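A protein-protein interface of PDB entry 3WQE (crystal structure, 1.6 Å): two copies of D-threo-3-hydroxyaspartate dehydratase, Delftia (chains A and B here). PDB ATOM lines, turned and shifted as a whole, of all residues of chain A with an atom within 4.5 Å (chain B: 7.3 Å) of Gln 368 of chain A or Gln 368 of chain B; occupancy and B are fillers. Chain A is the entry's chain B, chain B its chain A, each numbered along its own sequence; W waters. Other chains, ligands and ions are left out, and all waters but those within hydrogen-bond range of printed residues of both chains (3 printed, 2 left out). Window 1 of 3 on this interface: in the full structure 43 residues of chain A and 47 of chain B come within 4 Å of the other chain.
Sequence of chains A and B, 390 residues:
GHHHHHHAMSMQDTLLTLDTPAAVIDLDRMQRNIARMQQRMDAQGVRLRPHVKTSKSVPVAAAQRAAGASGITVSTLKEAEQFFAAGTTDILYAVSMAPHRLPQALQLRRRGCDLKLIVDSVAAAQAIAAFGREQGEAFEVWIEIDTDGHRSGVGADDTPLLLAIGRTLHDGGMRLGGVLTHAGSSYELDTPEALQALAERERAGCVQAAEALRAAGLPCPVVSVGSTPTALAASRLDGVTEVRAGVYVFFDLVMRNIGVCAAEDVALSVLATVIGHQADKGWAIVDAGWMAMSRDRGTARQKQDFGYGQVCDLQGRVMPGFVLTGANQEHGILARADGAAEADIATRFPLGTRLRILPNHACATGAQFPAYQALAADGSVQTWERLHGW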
ATOM      1  N   TRP A 290      16.681 -13.115  24.307  1.00  0.00           N
ATOM      2  CA  TRP A 290      17.653 -13.587  23.376  1.00  0.00           C
ATOM      3  C   TRP A 290      17.430 -13.094  21.948  1.00  0.00           C
ATOM      4  O   TRP A 290      18.340 -13.114  21.103  1.00  0.00           O
ATOM      5  CB  TRP A 290      17.790 -15.164  23.393  1.00  0.00           C
ATOM      6  CG  TRP A 290      16.520 -15.918  23.024  1.00  0.00           C
ATOM      7  CD1 TRP A 290      15.697 -16.593  23.885  1.00  0.00           C
ATOM      8  CD2 TRP A 290      15.911 -16.041  21.660  1.00  0.00           C
ATOM      9  NE1 TRP A 290      14.649 -17.192  23.194  1.00  0.00           N
ATOM     10  CE2 TRP A 290      14.734 -16.838  21.858  1.00  0.00           C
ATOM     11  CE3 TRP A 290      16.242 -15.631  20.352  1.00  0.00           C
ATOM     12  CZ2 TRP A 290      13.896 -17.115  20.776  1.00  0.00           C
ATOM     13  CZ3 TRP A 290      15.372 -15.936  19.254  1.00  0.00           C
ATOM     14  CH2 TRP A 290      14.201 -16.701  19.514  1.00  0.00           C
ATOM     15  N   MET A 291      16.188 -12.593  21.653  1.00  0.00           N
ATOM     16  CA  MET A 291      16.061 -12.008  20.324  1.00  0.00           C
ATOM     17  C   MET A 291      16.926 -10.729  20.210  1.00  0.00           C
ATOM     18  O   MET A 291      17.438 -10.470  19.119  1.00  0.00           O
ATOM     19  CB  MET A 291      14.548 -11.727  20.003  1.00  0.00           C
ATOM     20  CG  MET A 291      14.361 -11.205  18.561  1.00  0.00           C
ATOM     21  SD  MET A 291      14.689 -12.538  17.352  1.00  0.00           S
ATOM     22  CE  MET A 291      13.230 -13.620  17.691  1.00  0.00           C
ATOM     23  N   ALA A 292      17.138 -10.040  21.316  1.00  0.00           N
ATOM     24  CA  ALA A 292      18.080  -8.885  21.288  1.00  0.00           C
ATOM     25  C   ALA A 292      19.513  -9.317  21.478  1.00  0.00           C
ATOM     26  O   ALA A 292      20.414  -8.844  20.765  1.00  0.00           O
ATOM     27  CB  ALA A 292      17.729  -7.851  22.357  1.00  0.00           C
ATOM     28  N   SER A 294      20.912 -12.358  21.116  1.00  0.00           N
ATOM     29  CA  SER A 294      21.200 -13.611  20.461  1.00  0.00           C
ATOM     30  C   SER A 294      21.314 -14.729  21.551  1.00  0.00           C
ATOM     31  O   SER A 294      21.478 -14.483  22.755  1.00  0.00           O
ATOM     32  CB  SER A 294      22.430 -13.636  19.557  1.00  0.00           C
ATOM     33  OG  SER A 294      23.628 -13.995  20.341  1.00  0.00           O
ATOM     34  N   ALA A 364      27.326 -11.993  16.863  1.00  0.00           N
ATOM     35  CA  ALA A 364      25.972 -12.619  16.999  1.00  0.00           C
ATOM     36  C   ALA A 364      24.935 -11.624  17.462  1.00  0.00           C
ATOM     37  O   ALA A 364      23.799 -11.575  16.910  1.00  0.00           O
ATOM     38  CB  ALA A 364      26.082 -13.769  18.005  1.00  0.00           C
ATOM     39  N   THR A 365      25.310 -10.783  18.461  1.00  0.00           N
ATOM     40  CA  THR A 365      24.299  -9.765  18.944  1.00  0.00           C
ATOM     41  C   THR A 365      24.006  -8.801  17.833  1.00  0.00           C
ATOM     42  O   THR A 365      22.819  -8.444  17.628  1.00  0.00           O
ATOM     43  CB  THR A 365      24.873  -9.035  20.189  1.00  0.00           C
ATOM     44  OG1 THR A 365      25.039 -10.001  21.211  1.00  0.00           O
ATOM     45  CG2 THR A 365      23.950  -7.926  20.619  1.00  0.00           C
ATOM     46  N   GLY A 366      25.039  -8.330  17.102  1.00  0.00           N
ATOM     47  CA  GLY A 366      24.751  -7.266  16.088  1.00  0.00           C
ATOM     48  C   GLY A 366      23.736  -7.760  15.035  1.00  0.00           C
ATOM     49  O   GLY A 366      22.917  -6.965  14.556  1.00  0.00           O
ATOM     50  N   ALA A 367      23.840  -9.049  14.658  1.00  0.00           N
ATOM     51  CA  ALA A 367      22.980  -9.519  13.593  1.00  0.00           C
ATOM     52  C   ALA A 367      21.500  -9.572  13.976  1.00  0.00           C
ATOM     53  O   ALA A 367      20.663  -9.752  13.101  1.00  0.00           O
ATOM     54  CB  ALA A 367      23.468 -10.960  13.234  1.00  0.00           C
ATOM     55  N   GLN A 368      21.212  -9.452  15.270  1.00  0.00           N
ATOM     56  CA  GLN A 368      19.809  -9.412  15.667  1.00  0.00           C
ATOM     57  C   GLN A 368      19.133  -8.080  15.360  1.00  0.00           C
ATOM     58  O   GLN A 368      17.911  -7.943  15.484  1.00  0.00           O
ATOM     59  CB  GLN A 368      19.721  -9.682  17.145  1.00  0.00           C
ATOM     60  CG  GLN A 368      20.323 -11.068  17.412  1.00  0.00           C
ATOM     61  CD  GLN A 368      19.579 -12.151  16.697  1.00  0.00           C
ATOM     62  OE1 GLN A 368      19.969 -12.618  15.633  1.00  0.00           O
ATOM     63  NE2 GLN A 368      18.466 -12.627  17.343  1.00  0.00           N
ATOM     64  N   PHE A 369      19.934  -7.077  14.921  1.00  0.00           N
ATOM     65  CA  PHE A 369      19.349  -5.697  14.749  1.00  0.00           C
ATOM     66  C   PHE A 369      19.377  -5.220  13.309  1.00  0.00           C
ATOM     67  O   PHE A 369      20.384  -5.425  12.623  1.00  0.00           O
ATOM     68  CB  PHE A 369      20.148  -4.692  15.632  1.00  0.00           C
ATOM     69  CG  PHE A 369      19.904  -4.888  17.092  1.00  0.00           C
ATOM     70  CD1 PHE A 369      20.724  -5.861  17.753  1.00  0.00           C
ATOM     71  CD2 PHE A 369      18.928  -4.198  17.775  1.00  0.00           C
ATOM     72  CE1 PHE A 369      20.510  -6.104  19.139  1.00  0.00           C
ATOM     73  CE2 PHE A 369      18.690  -4.462  19.153  1.00  0.00           C
ATOM     74  CZ  PHE A 369      19.539  -5.379  19.755  1.00  0.00           C
ATOM     75  N   PRO A 370      18.325  -4.578  12.820  1.00  0.00           N
ATOM     76  CA  PRO A 370      18.358  -3.953  11.492  1.00  0.00           C
ATOM     77  C   PRO A 370      19.389  -2.809  11.431  1.00  0.00           C
ATOM     78  O   PRO A 370      19.868  -2.568  10.327  1.00  0.00           O
ATOM     79  CB  PRO A 370      16.952  -3.329  11.358  1.00  0.00           C
ATOM     80  CG  PRO A 370      16.084  -4.214  12.234  1.00  0.00           C
ATOM     81  CD  PRO A 370      16.945  -4.552  13.416  1.00  0.00           C
ATOM     82  N   HIS A 388      21.088  -7.781   6.821  1.00  0.00           N
ATOM     83  CA  HIS A 388      20.527  -9.038   7.370  1.00  0.00           C
ATOM     84  C   HIS A 388      20.264  -9.978   6.212  1.00  0.00           C
ATOM     85  O   HIS A 388      19.790  -9.589   5.165  1.00  0.00           O
ATOM     86  CB  HIS A 388      19.150  -8.646   7.999  1.00  0.00           C
ATOM     87  CG  HIS A 388      18.474  -9.791   8.726  1.00  0.00           C
ATOM     88  ND1 HIS A 388      17.145 -10.079   8.501  1.00  0.00           N
ATOM     89  CD2 HIS A 388      18.964 -10.679   9.645  1.00  0.00           C
ATOM     90  CE1 HIS A 388      16.809 -11.052   9.379  1.00  0.00           C
ATOM     91  NE2 HIS A 388      17.884 -11.422  10.063  1.00  0.00           N
ATOM     92  N   TRP A 390      21.001 -13.026   3.265  1.00  0.00           N
ATOM     93  CA  TRP A 390      21.902 -13.498   2.162  1.00  0.00           C
ATOM     94  C   TRP A 390      21.489 -12.969   0.822  1.00  0.00           C
ATOM     95  O   TRP A 390      20.428 -12.280   0.749  1.00  0.00           O
ATOM     96  CB  TRP A 390      21.928 -15.073   2.122  1.00  0.00           C
ATOM     97  CG  TRP A 390      22.524 -15.615   3.409  1.00  0.00           C
ATOM     98  CD1 TRP A 390      23.827 -15.985   3.640  1.00  0.00           C
ATOM     99  CD2 TRP A 390      21.814 -15.834   4.691  1.00  0.00           C
ATOM    100  NE1 TRP A 390      23.982 -16.399   4.939  1.00  0.00           N
ATOM    101  CE2 TRP A 390      22.782 -16.352   5.623  1.00  0.00           C
ATOM    102  CE3 TRP A 390      20.461 -15.708   5.123  1.00  0.00           C
ATOM    103  CZ2 TRP A 390      22.445 -16.618   6.979  1.00  0.00           C
ATOM    104  CZ3 TRP A 390      20.186 -15.993   6.478  1.00  0.00           C
ATOM    105  CH2 TRP A 390      21.163 -16.406   7.383  1.00  0.00           C
ATOM    106  OXT TRP A 390      22.246 -13.302  -0.168  1.00  0.00           O
ATOM    107  N   ALA B  23      15.421 -20.531   4.420  1.00  0.00           N
ATOM    108  CA  ALA B  23      14.464 -21.080   5.372  1.00  0.00           C
ATOM    109  C   ALA B  23      13.243 -21.528   4.638  1.00  0.00           C
ATOM    110  O   ALA B  23      12.513 -20.704   4.091  1.00  0.00           O
ATOM    111  CB  ALA B  23      14.113 -19.993   6.430  1.00  0.00           C
ATOM    112  N   GLY B 289      25.730 -21.933   8.770  1.00  0.00           N
ATOM    113  CA  GLY B 289      26.343 -21.878  10.139  1.00  0.00           C
ATOM    114  C   GLY B 289      25.321 -21.333  11.131  1.00  0.00           C
ATOM    115  O   GLY B 289      24.120 -21.422  10.925  1.00  0.00           O
ATOM    116  N   TRP B 290      25.855 -20.820  12.271  1.00  0.00           N
ATOM    117  CA  TRP B 290      24.881 -20.325  13.284  1.00  0.00           C
ATOM    118  C   TRP B 290      24.199 -19.078  12.782  1.00  0.00           C
ATOM    119  O   TRP B 290      23.148 -18.700  13.295  1.00  0.00           O
ATOM    120  CB  TRP B 290      25.521 -20.161  14.701  1.00  0.00           C
ATOM    121  CG  TRP B 290      26.678 -19.159  14.769  1.00  0.00           C
ATOM    122  CD1 TRP B 290      28.013 -19.408  14.966  1.00  0.00           C
ATOM    123  CD2 TRP B 290      26.538 -17.679  14.733  1.00  0.00           C
ATOM    124  NE1 TRP B 290      28.738 -18.240  15.008  1.00  0.00           N
ATOM    125  CE2 TRP B 290      27.909 -17.198  14.902  1.00  0.00           C
ATOM    126  CE3 TRP B 290      25.464 -16.783  14.622  1.00  0.00           C
ATOM    127  CZ2 TRP B 290      28.201 -15.866  14.839  1.00  0.00           C
ATOM    128  CZ3 TRP B 290      25.785 -15.348  14.544  1.00  0.00           C
ATOM    129  CH2 TRP B 290      27.175 -14.936  14.687  1.00  0.00           C
ATOM    130  N   MET B 291      24.740 -18.323  11.780  1.00  0.00           N
ATOM    131  CA  MET B 291      23.937 -17.202  11.319  1.00  0.00           C
ATOM    132  C   MET B 291      22.636 -17.670  10.660  1.00  0.00           C
ATOM    133  O   MET B 291      21.650 -16.978  10.642  1.00  0.00           O
ATOM    134  CB  MET B 291      24.737 -16.334  10.355  1.00  0.00           C
ATOM    135  CG  MET B 291      24.084 -15.003   9.962  1.00  0.00           C
ATOM    136  SD  MET B 291      23.830 -13.892  11.385  1.00  0.00           S
ATOM    137  CE  MET B 291      25.524 -13.299  11.511  1.00  0.00           C
ATOM    138  N   ALA B 292      22.689 -18.864  10.034  1.00  0.00           N
ATOM    139  CA  ALA B 292      21.457 -19.448   9.496  1.00  0.00           C
ATOM    140  C   ALA B 292      20.654 -20.153  10.615  1.00  0.00           C
ATOM    141  O   ALA B 292      19.419 -19.990  10.680  1.00  0.00           O
ATOM    142  CB  ALA B 292      21.788 -20.459   8.370  1.00  0.00           C
ATOM    143  N   MET B 293      21.301 -21.023  11.390  1.00  0.00           N
ATOM    144  CA  MET B 293      20.531 -21.804  12.330  1.00  0.00           C
ATOM    145  C   MET B 293      20.128 -21.094  13.593  1.00  0.00           C
ATOM    146  O   MET B 293      19.220 -21.525  14.295  1.00  0.00           O
ATOM    147  CB  MET B 293      21.331 -23.073  12.749  1.00  0.00           C
ATOM    148  CG  MET B 293      21.734 -23.997  11.589  1.00  0.00           C
ATOM    149  SD  MET B 293      20.406 -24.378  10.420  1.00  0.00           S
ATOM    150  CE  MET B 293      19.138 -25.145  11.519  1.00  0.00           C
ATOM    151  N   SER B 294      20.805 -19.985  13.891  1.00  0.00           N
ATOM    152  CA  SER B 294      20.867 -19.356  15.223  1.00  0.00           C
ATOM    153  C   SER B 294      21.816 -20.118  16.099  1.00  0.00           C
ATOM    154  O   SER B 294      22.100 -21.299  15.893  1.00  0.00           O
ATOM    155  CB  SER B 294      19.452 -19.099  15.867  1.00  0.00           C
ATOM    156  OG  SER B 294      19.133 -20.235  16.672  1.00  0.00           O
ATOM    157  N   ARG B 295      22.149 -19.444  17.227  1.00  0.00           N
ATOM    158  CA  ARG B 295      22.952 -20.127  18.275  1.00  0.00           C
ATOM    159  C   ARG B 295      22.126 -20.974  19.246  1.00  0.00           C
ATOM    160  O   ARG B 295      22.699 -21.482  20.172  1.00  0.00           O
ATOM    161  CB  ARG B 295      23.717 -19.042  19.083  1.00  0.00           C
ATOM    162  CG  ARG B 295      25.063 -18.601  18.402  1.00  0.00           C
ATOM    163  CD  ARG B 295      26.082 -19.747  18.476  1.00  0.00           C
ATOM    164  NE  ARG B 295      27.397 -19.129  18.525  1.00  0.00           N
ATOM    165  CZ  ARG B 295      28.488 -19.822  18.352  1.00  0.00           C
ATOM    166  NH1 ARG B 295      28.433 -21.087  17.922  1.00  0.00           N
ATOM    167  NH2 ARG B 295      29.707 -19.190  18.526  1.00  0.00           N
ATOM    168  N   ALA B 362      12.331 -23.349  16.367  1.00  0.00           N
ATOM    169  CA  ALA B 362      11.910 -22.706  15.140  1.00  0.00           C
ATOM    170  C   ALA B 362      11.883 -21.166  15.277  1.00  0.00           C
ATOM    171  O   ALA B 362      12.216 -20.472  14.314  1.00  0.00           O
ATOM    172  CB  ALA B 362      10.477 -23.235  14.768  1.00  0.00           C
ATOM    173  N   CYS B 363      11.488 -20.652  16.438  1.00  0.00           N
ATOM    174  CA  CYS B 363      11.352 -19.179  16.571  1.00  0.00           C
ATOM    175  C   CYS B 363      12.725 -18.515  16.423  1.00  0.00           C
ATOM    176  O   CYS B 363      12.816 -17.424  15.860  1.00  0.00           O
ATOM    177  CB  CYS B 363      10.928 -18.886  18.023  1.00  0.00           C
ATOM    178  SG  CYS B 363       9.434 -19.895  18.519  1.00  0.00           S
ATOM    179  N   ALA B 364      13.798 -19.216  16.881  1.00  0.00           N
ATOM    180  CA  ALA B 364      15.126 -18.615  16.849  1.00  0.00           C
ATOM    181  C   ALA B 364      15.677 -18.697  15.391  1.00  0.00           C
ATOM    182  O   ALA B 364      16.272 -17.760  14.892  1.00  0.00           O
ATOM    183  CB  ALA B 364      16.044 -19.400  17.828  1.00  0.00           C
ATOM    184  N   THR B 365      15.496 -19.912  14.766  1.00  0.00           N
ATOM    185  CA  THR B 365      16.063 -20.061  13.394  1.00  0.00           C
ATOM    186  C   THR B 365      15.364 -19.134  12.423  1.00  0.00           C
ATOM    187  O   THR B 365      15.982 -18.442  11.620  1.00  0.00           O
ATOM    188  CB  THR B 365      15.847 -21.522  12.994  1.00  0.00           C
ATOM    189  OG1 THR B 365      16.713 -22.331  13.765  1.00  0.00           O
ATOM    190  CG2 THR B 365      16.316 -21.721  11.503  1.00  0.00           C
ATOM    191  N   GLY B 366      14.015 -19.016  12.528  1.00  0.00           N
ATOM    192  CA  GLY B 366      13.234 -18.161  11.561  1.00  0.00           C
ATOM    193  C   GLY B 366      13.703 -16.700  11.605  1.00  0.00           C
ATOM    194  O   GLY B 366      13.745 -16.076  10.577  1.00  0.00           O
ATOM    195  N   ALA B 367      14.046 -16.243  12.837  1.00  0.00           N
ATOM    196  CA  ALA B 367      14.407 -14.860  12.979  1.00  0.00           C
ATOM    197  C   ALA B 367      15.725 -14.506  12.282  1.00  0.00           C
ATOM    198  O   ALA B 367      16.003 -13.309  12.060  1.00  0.00           O
ATOM    199  CB  ALA B 367      14.530 -14.503  14.467  1.00  0.00           C
ATOM    200  N   GLN B 368      16.497 -15.524  11.914  1.00  0.00           N
ATOM    201  CA  GLN B 368      17.730 -15.252  11.171  1.00  0.00           C
ATOM    202  C   GLN B 368      17.496 -14.897   9.706  1.00  0.00           C
ATOM    203  O   GLN B 368      18.440 -14.481   9.020  1.00  0.00           O
ATOM    204  CB  GLN B 368      18.633 -16.493  11.243  1.00  0.00           C
ATOM    205  CG  GLN B 368      19.051 -16.768  12.675  1.00  0.00           C
ATOM    206  CD  GLN B 368      19.702 -15.659  13.377  1.00  0.00           C
ATOM    207  OE1 GLN B 368      19.055 -14.821  14.023  1.00  0.00           O
ATOM    208  NE2 GLN B 368      21.033 -15.683  13.400  1.00  0.00           N
ATOM    209  N   PHE B 369      16.239 -15.067   9.193  1.00  0.00           N
ATOM    210  CA  PHE B 369      16.054 -14.896   7.761  1.00  0.00           C
ATOM    211  C   PHE B 369      15.122 -13.726   7.431  1.00  0.00           C
ATOM    212  O   PHE B 369      14.098 -13.542   8.180  1.00  0.00           O
ATOM    213  CB  PHE B 369      15.342 -16.180   7.200  1.00  0.00           C
ATOM    214  CG  PHE B 369      16.316 -17.369   7.177  1.00  0.00           C
ATOM    215  CD1 PHE B 369      16.489 -18.125   8.339  1.00  0.00           C
ATOM    216  CD2 PHE B 369      17.071 -17.604   6.031  1.00  0.00           C
ATOM    217  CE1 PHE B 369      17.428 -19.151   8.311  1.00  0.00           C
ATOM    218  CE2 PHE B 369      18.027 -18.679   6.017  1.00  0.00           C
ATOM    219  CZ  PHE B 369      18.171 -19.357   7.160  1.00  0.00           C
ATOM    220  N   PRO B 370      15.378 -12.960   6.415  1.00  0.00           N
ATOM    221  CA  PRO B 370      14.461 -11.928   5.991  1.00  0.00           C
ATOM    222  C   PRO B 370      13.098 -12.507   5.511  1.00  0.00           C
ATOM    223  O   PRO B 370      12.100 -11.730   5.539  1.00  0.00           O
ATOM    224  CB  PRO B 370      15.181 -11.268   4.792  1.00  0.00           C
ATOM    225  CG  PRO B 370      16.673 -11.556   5.101  1.00  0.00           C
ATOM    226  CD  PRO B 370      16.729 -12.901   5.727  1.00  0.00           C
ATOM    227  N   ALA B 371      13.082 -13.765   5.118  1.00  0.00           N
ATOM    228  CA  ALA B 371      11.853 -14.337   4.507  1.00  0.00           C
ATOM    229  C   ALA B 371      12.018 -15.845   4.567  1.00  0.00           C
ATOM    230  O   ALA B 371      13.139 -16.409   4.647  1.00  0.00           O
ATOM    231  CB  ALA B 371      11.665 -13.897   3.056  1.00  0.00           C
ATOM    232  N   TYR B 372      10.803 -16.449   4.484  1.00  0.00           N
ATOM    233  CA  TYR B 372      10.695 -17.924   4.255  1.00  0.00           C
ATOM    234  C   TYR B 372      10.500 -18.185   2.773  1.00  0.00           C
ATOM    235  O   TYR B 372       9.979 -17.388   2.008  1.00  0.00           O
ATOM    236  CB  TYR B 372       9.493 -18.519   5.003  1.00  0.00           C
ATOM    237  CG  TYR B 372       9.553 -18.314   6.502  1.00  0.00           C
ATOM    238  CD1 TYR B 372      10.331 -19.161   7.339  1.00  0.00           C
ATOM    239  CD2 TYR B 372       8.817 -17.260   7.086  1.00  0.00           C
ATOM    240  CE1 TYR B 372      10.358 -19.024   8.739  1.00  0.00           C
ATOM    241  CE2 TYR B 372       8.875 -17.093   8.462  1.00  0.00           C
ATOM    242  CZ  TYR B 372       9.664 -17.915   9.278  1.00  0.00           C
ATOM    243  OH  TYR B 372       9.745 -17.813  10.630  1.00  0.00           O
ATOM    244  N   ARG B 386       9.185 -11.959   6.386  1.00  0.00           N
ATOM    245  CA  ARG B 386       8.848 -11.868   7.803  1.00  0.00           C
ATOM    246  C   ARG B 386       9.565 -10.669   8.464  1.00  0.00           C
ATOM    247  O   ARG B 386      10.531 -10.081   7.845  1.00  0.00           O
ATOM    248  CB  ARG B 386       9.189 -13.158   8.568  1.00  0.00           C
ATOM    249  CG  ARG B 386      10.737 -13.488   8.505  1.00  0.00           C
ATOM    250  CD  ARG B 386      11.072 -14.438   9.630  1.00  0.00           C
ATOM    251  NE  ARG B 386      11.129 -13.651  10.930  1.00  0.00           N
ATOM    252  CZ  ARG B 386      10.995 -14.209  12.131  1.00  0.00           C
ATOM    253  NH1 ARG B 386      11.154 -13.462  13.217  1.00  0.00           N
ATOM    254  NH2 ARG B 386      10.540 -15.499  12.292  1.00  0.00           N
ATOM    255  N   HIS B 388      11.839  -8.333  11.124  1.00  0.00           N
ATOM    256  CA  HIS B 388      13.078  -8.336  11.890  1.00  0.00           C
ATOM    257  C   HIS B 388      13.100  -7.012  12.677  1.00  0.00           C
ATOM    258  O   HIS B 388      12.773  -5.934  12.142  1.00  0.00           O
ATOM    259  CB  HIS B 388      14.244  -8.289  10.840  1.00  0.00           C
ATOM    260  CG  HIS B 388      15.610  -8.419  11.451  1.00  0.00           C
ATOM    261  ND1 HIS B 388      16.676  -7.597  11.003  1.00  0.00           N
ATOM    262  CD2 HIS B 388      16.095  -9.282  12.327  1.00  0.00           C
ATOM    263  CE1 HIS B 388      17.755  -7.993  11.658  1.00  0.00           C
ATOM    264  NE2 HIS B 388      17.435  -9.023  12.448  1.00  0.00           N
ATOM    265  N   GLY B 389      13.549  -7.124  13.917  1.00  0.00           N
ATOM    266  CA  GLY B 389      13.744  -5.893  14.715  1.00  0.00           C
ATOM    267  C   GLY B 389      12.576  -5.428  15.571  1.00  0.00           C
ATOM    268  O   GLY B 389      11.697  -6.239  15.867  1.00  0.00           O
ATOM    269  N   TRP B 390      12.608  -4.166  15.932  1.00  0.00           N
ATOM    270  CA  TRP B 390      11.667  -3.619  16.886  1.00  0.00           C
ATOM    271  C   TRP B 390      11.179  -2.302  16.369  1.00  0.00           C
ATOM    272  O   TRP B 390      11.706  -1.707  15.388  1.00  0.00           O
ATOM    273  CB  TRP B 390      12.349  -3.365  18.261  1.00  0.00           C
ATOM    274  CG  TRP B 390      12.747  -4.650  18.912  1.00  0.00           C
ATOM    275  CD1 TRP B 390      12.031  -5.410  19.844  1.00  0.00           C
ATOM    276  CD2 TRP B 390      13.952  -5.403  18.662  1.00  0.00           C
ATOM    277  NE1 TRP B 390      12.691  -6.507  20.155  1.00  0.00           N
ATOM    278  CE2 TRP B 390      13.861  -6.612  19.471  1.00  0.00           C
ATOM    279  CE3 TRP B 390      15.096  -5.232  17.809  1.00  0.00           C
ATOM    280  CZ2 TRP B 390      14.849  -7.583  19.474  1.00  0.00           C
ATOM    281  CZ3 TRP B 390      16.063  -6.267  17.836  1.00  0.00           C
ATOM    282  CH2 TRP B 390      15.933  -7.431  18.607  1.00  0.00           C
ATOM    283  OXT TRP B 390      10.210  -1.793  16.973  1.00  0.00           O
HETATM  284  O   HOH W   1      13.891  -9.296  15.655  1.00  0.00           O
HETATM  285  O   HOH W   2      17.549 -15.661  16.213  1.00  0.00           O
HETATM  286  O   HOH W   3      22.552 -13.683  15.545  1.00  0.00           O
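Met 291 of chain A touches Trp 390 of chain B, and with the chains exchanged Trp 390 of chain A touches Met 291 of chain B.
Phe 369 of chain A touches His 388 of chain B, and with the chains exchanged His 388 of chain A touches Phe 369 of chain B.
Positions printed for both chains: 290, 291, 292, 294, 364, 365, 366, 367, 368, 369, 370, 388 and 390.
The backbone carbonyl oxygen (O) of Met 291 of chain B lies within hydrogen-bond range of the side-chain amide nitrogen (NE2) of Gln 368 of chain B (3.1 Å).
NE2 of Gln 368 of chain A lies within hydrogen-bond range of O of Met 291 of chain A (3.0 Å).
The backbone NH of Arg 386 of chain B is in hydrogen-bond range of the backbone carbonyl oxygen of Pro 370 of chain B, at 3.0 Å.
Hydrophobic or aromatic side chains of chain A within 4 Å of the printed part of chain B: Trp 290, Met 291, Ala 364, Ala 367, Phe 369, Pro 370, His 388 and Trp 390.
Of the 23 printed residues of chain B, 12 touch a printed residue of chain A.
Hydrophobic or aromatic side chains of chain B within 4 Å of the printed part of chain A: Trp 290, Met 291, Ala 364, Ala 367, Phe 369, Pro 370, His 388 and Trp 390.
Among the printed residues, 24 pairs touch across the chains.
Among the printed residues, no Asp or Glu carboxylate lies within 4 Å of a Lys or Arg side-chain nitrogen of the other chain.
Among the printed residues, pairs that only touch across the chains: Trp 390 of chain A with Met 291 of chain B (3.3 Å), Trp 290 of chain A with Ala 364 of chain B (3.4 Å), Gln 368 of chain A with Trp 390 of chain B (3.4 Å), Met 291 of chain A with Trp 390 of chain B (3.4 Å), Trp 390 of chain A with Gln 368 of chain B (3.4 Å), Phe 369 of chain A with Trp 390 of chain B (3.4 Å), Trp 390 of chain A with Phe 369 of chain B (3.5 Å), Ala 367 of chain A with Met 291 of chain B (3.5 Å), Ala 364 of chain A with Trp 290 of chain B (3.5 Å), Met 291 of chain A with Ala 367 of chain B (3.5 Å), Phe 369 of chain A with His 388 of chain B (3.6 Å), Pro 370 of chain A with His 388 of chain B (3.6 Å), His 388 of chain A with Pro 370 of chain B (3.7 Å), Pro 370 of chain A with Gly 389 of chain B (3.7 Å), His 388 of chain A with Phe 369 of chain B (3.7 Å), Trp 390 of chain A with Ala 292 of chain B (3.7 Å), Ala 292 of chain A with Trp 390 of chain B (3.7 Å) and Trp 290 of chain A with Cys 363 of chain B (3.9 Å).
Of the printed residues of chain B, Gln 368 of chain A touches Gln 368 (2.9 Å), His 388 (3.3 Å) and Trp 390 (3.4 Å).
Of the printed residues of chain B, Ala 367 of chain A touches Met 291 (3.5 Å) and His 388 (3.4 Å).
Printed residues of chain A within 4 Å of His 388 of chain B: Ala 367, Gln 368, Phe 369, Pro 370 and His 388.
Of the printed residues of chain A, Ala 292 of chain B touches Trp 390.
Ala 23 of chain B touches none of the printed residues of chain A.
The nearest printed residue of chain A that does not touch Gln 368 of chain B is Ala 367 of chain A (5.3 Å).
OE1 of Gln 368 of chain B lies close to OE1 of Gln 368 of chain A (2.9 Å).
O of Ala 367 of chain A sits at hydrogen-bond distance from NE2 of His 388 of chain B.
NE2 of His 388 of chain B sits at hydrogen-bond distance from O of Gln 368 of chain A (3.3 Å).
O of Ala 367 of chain B is in hydrogen-bond range of NE2 of His 388 of chain A (3.3 Å).
A ring nitrogen (NE2) of His 388 of chain B sits at hydrogen-bond distance from a ring nitrogen (NE2) of His 388 of chain A.
A ring nitrogen (NE2) of His 388 of chain A lies within hydrogen-bond range of the backbone carbonyl oxygen of Gln 368 of chain B (3.3 Å).
Water W2 lies within hydrogen-bond range of the side-chain amide oxygen of Gln 368 of chain B (2.8 Å), the backbone carbonyl oxygen of Ala 364 of chain B (2.8 Å) and the side-chain amide nitrogen of Gln 368 of chain A (3.4 Å).
Water W3 lies within hydrogen-bond range of OE1 of Gln 368 of chain A (2.8 Å), O of Ala 364 of chain A (2.8 Å) and NE2 of Gln 368 of chain B (3.3 Å).
Water W1 bridges N of Gly 389 of chain B and SD of Met 291 of chain A.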
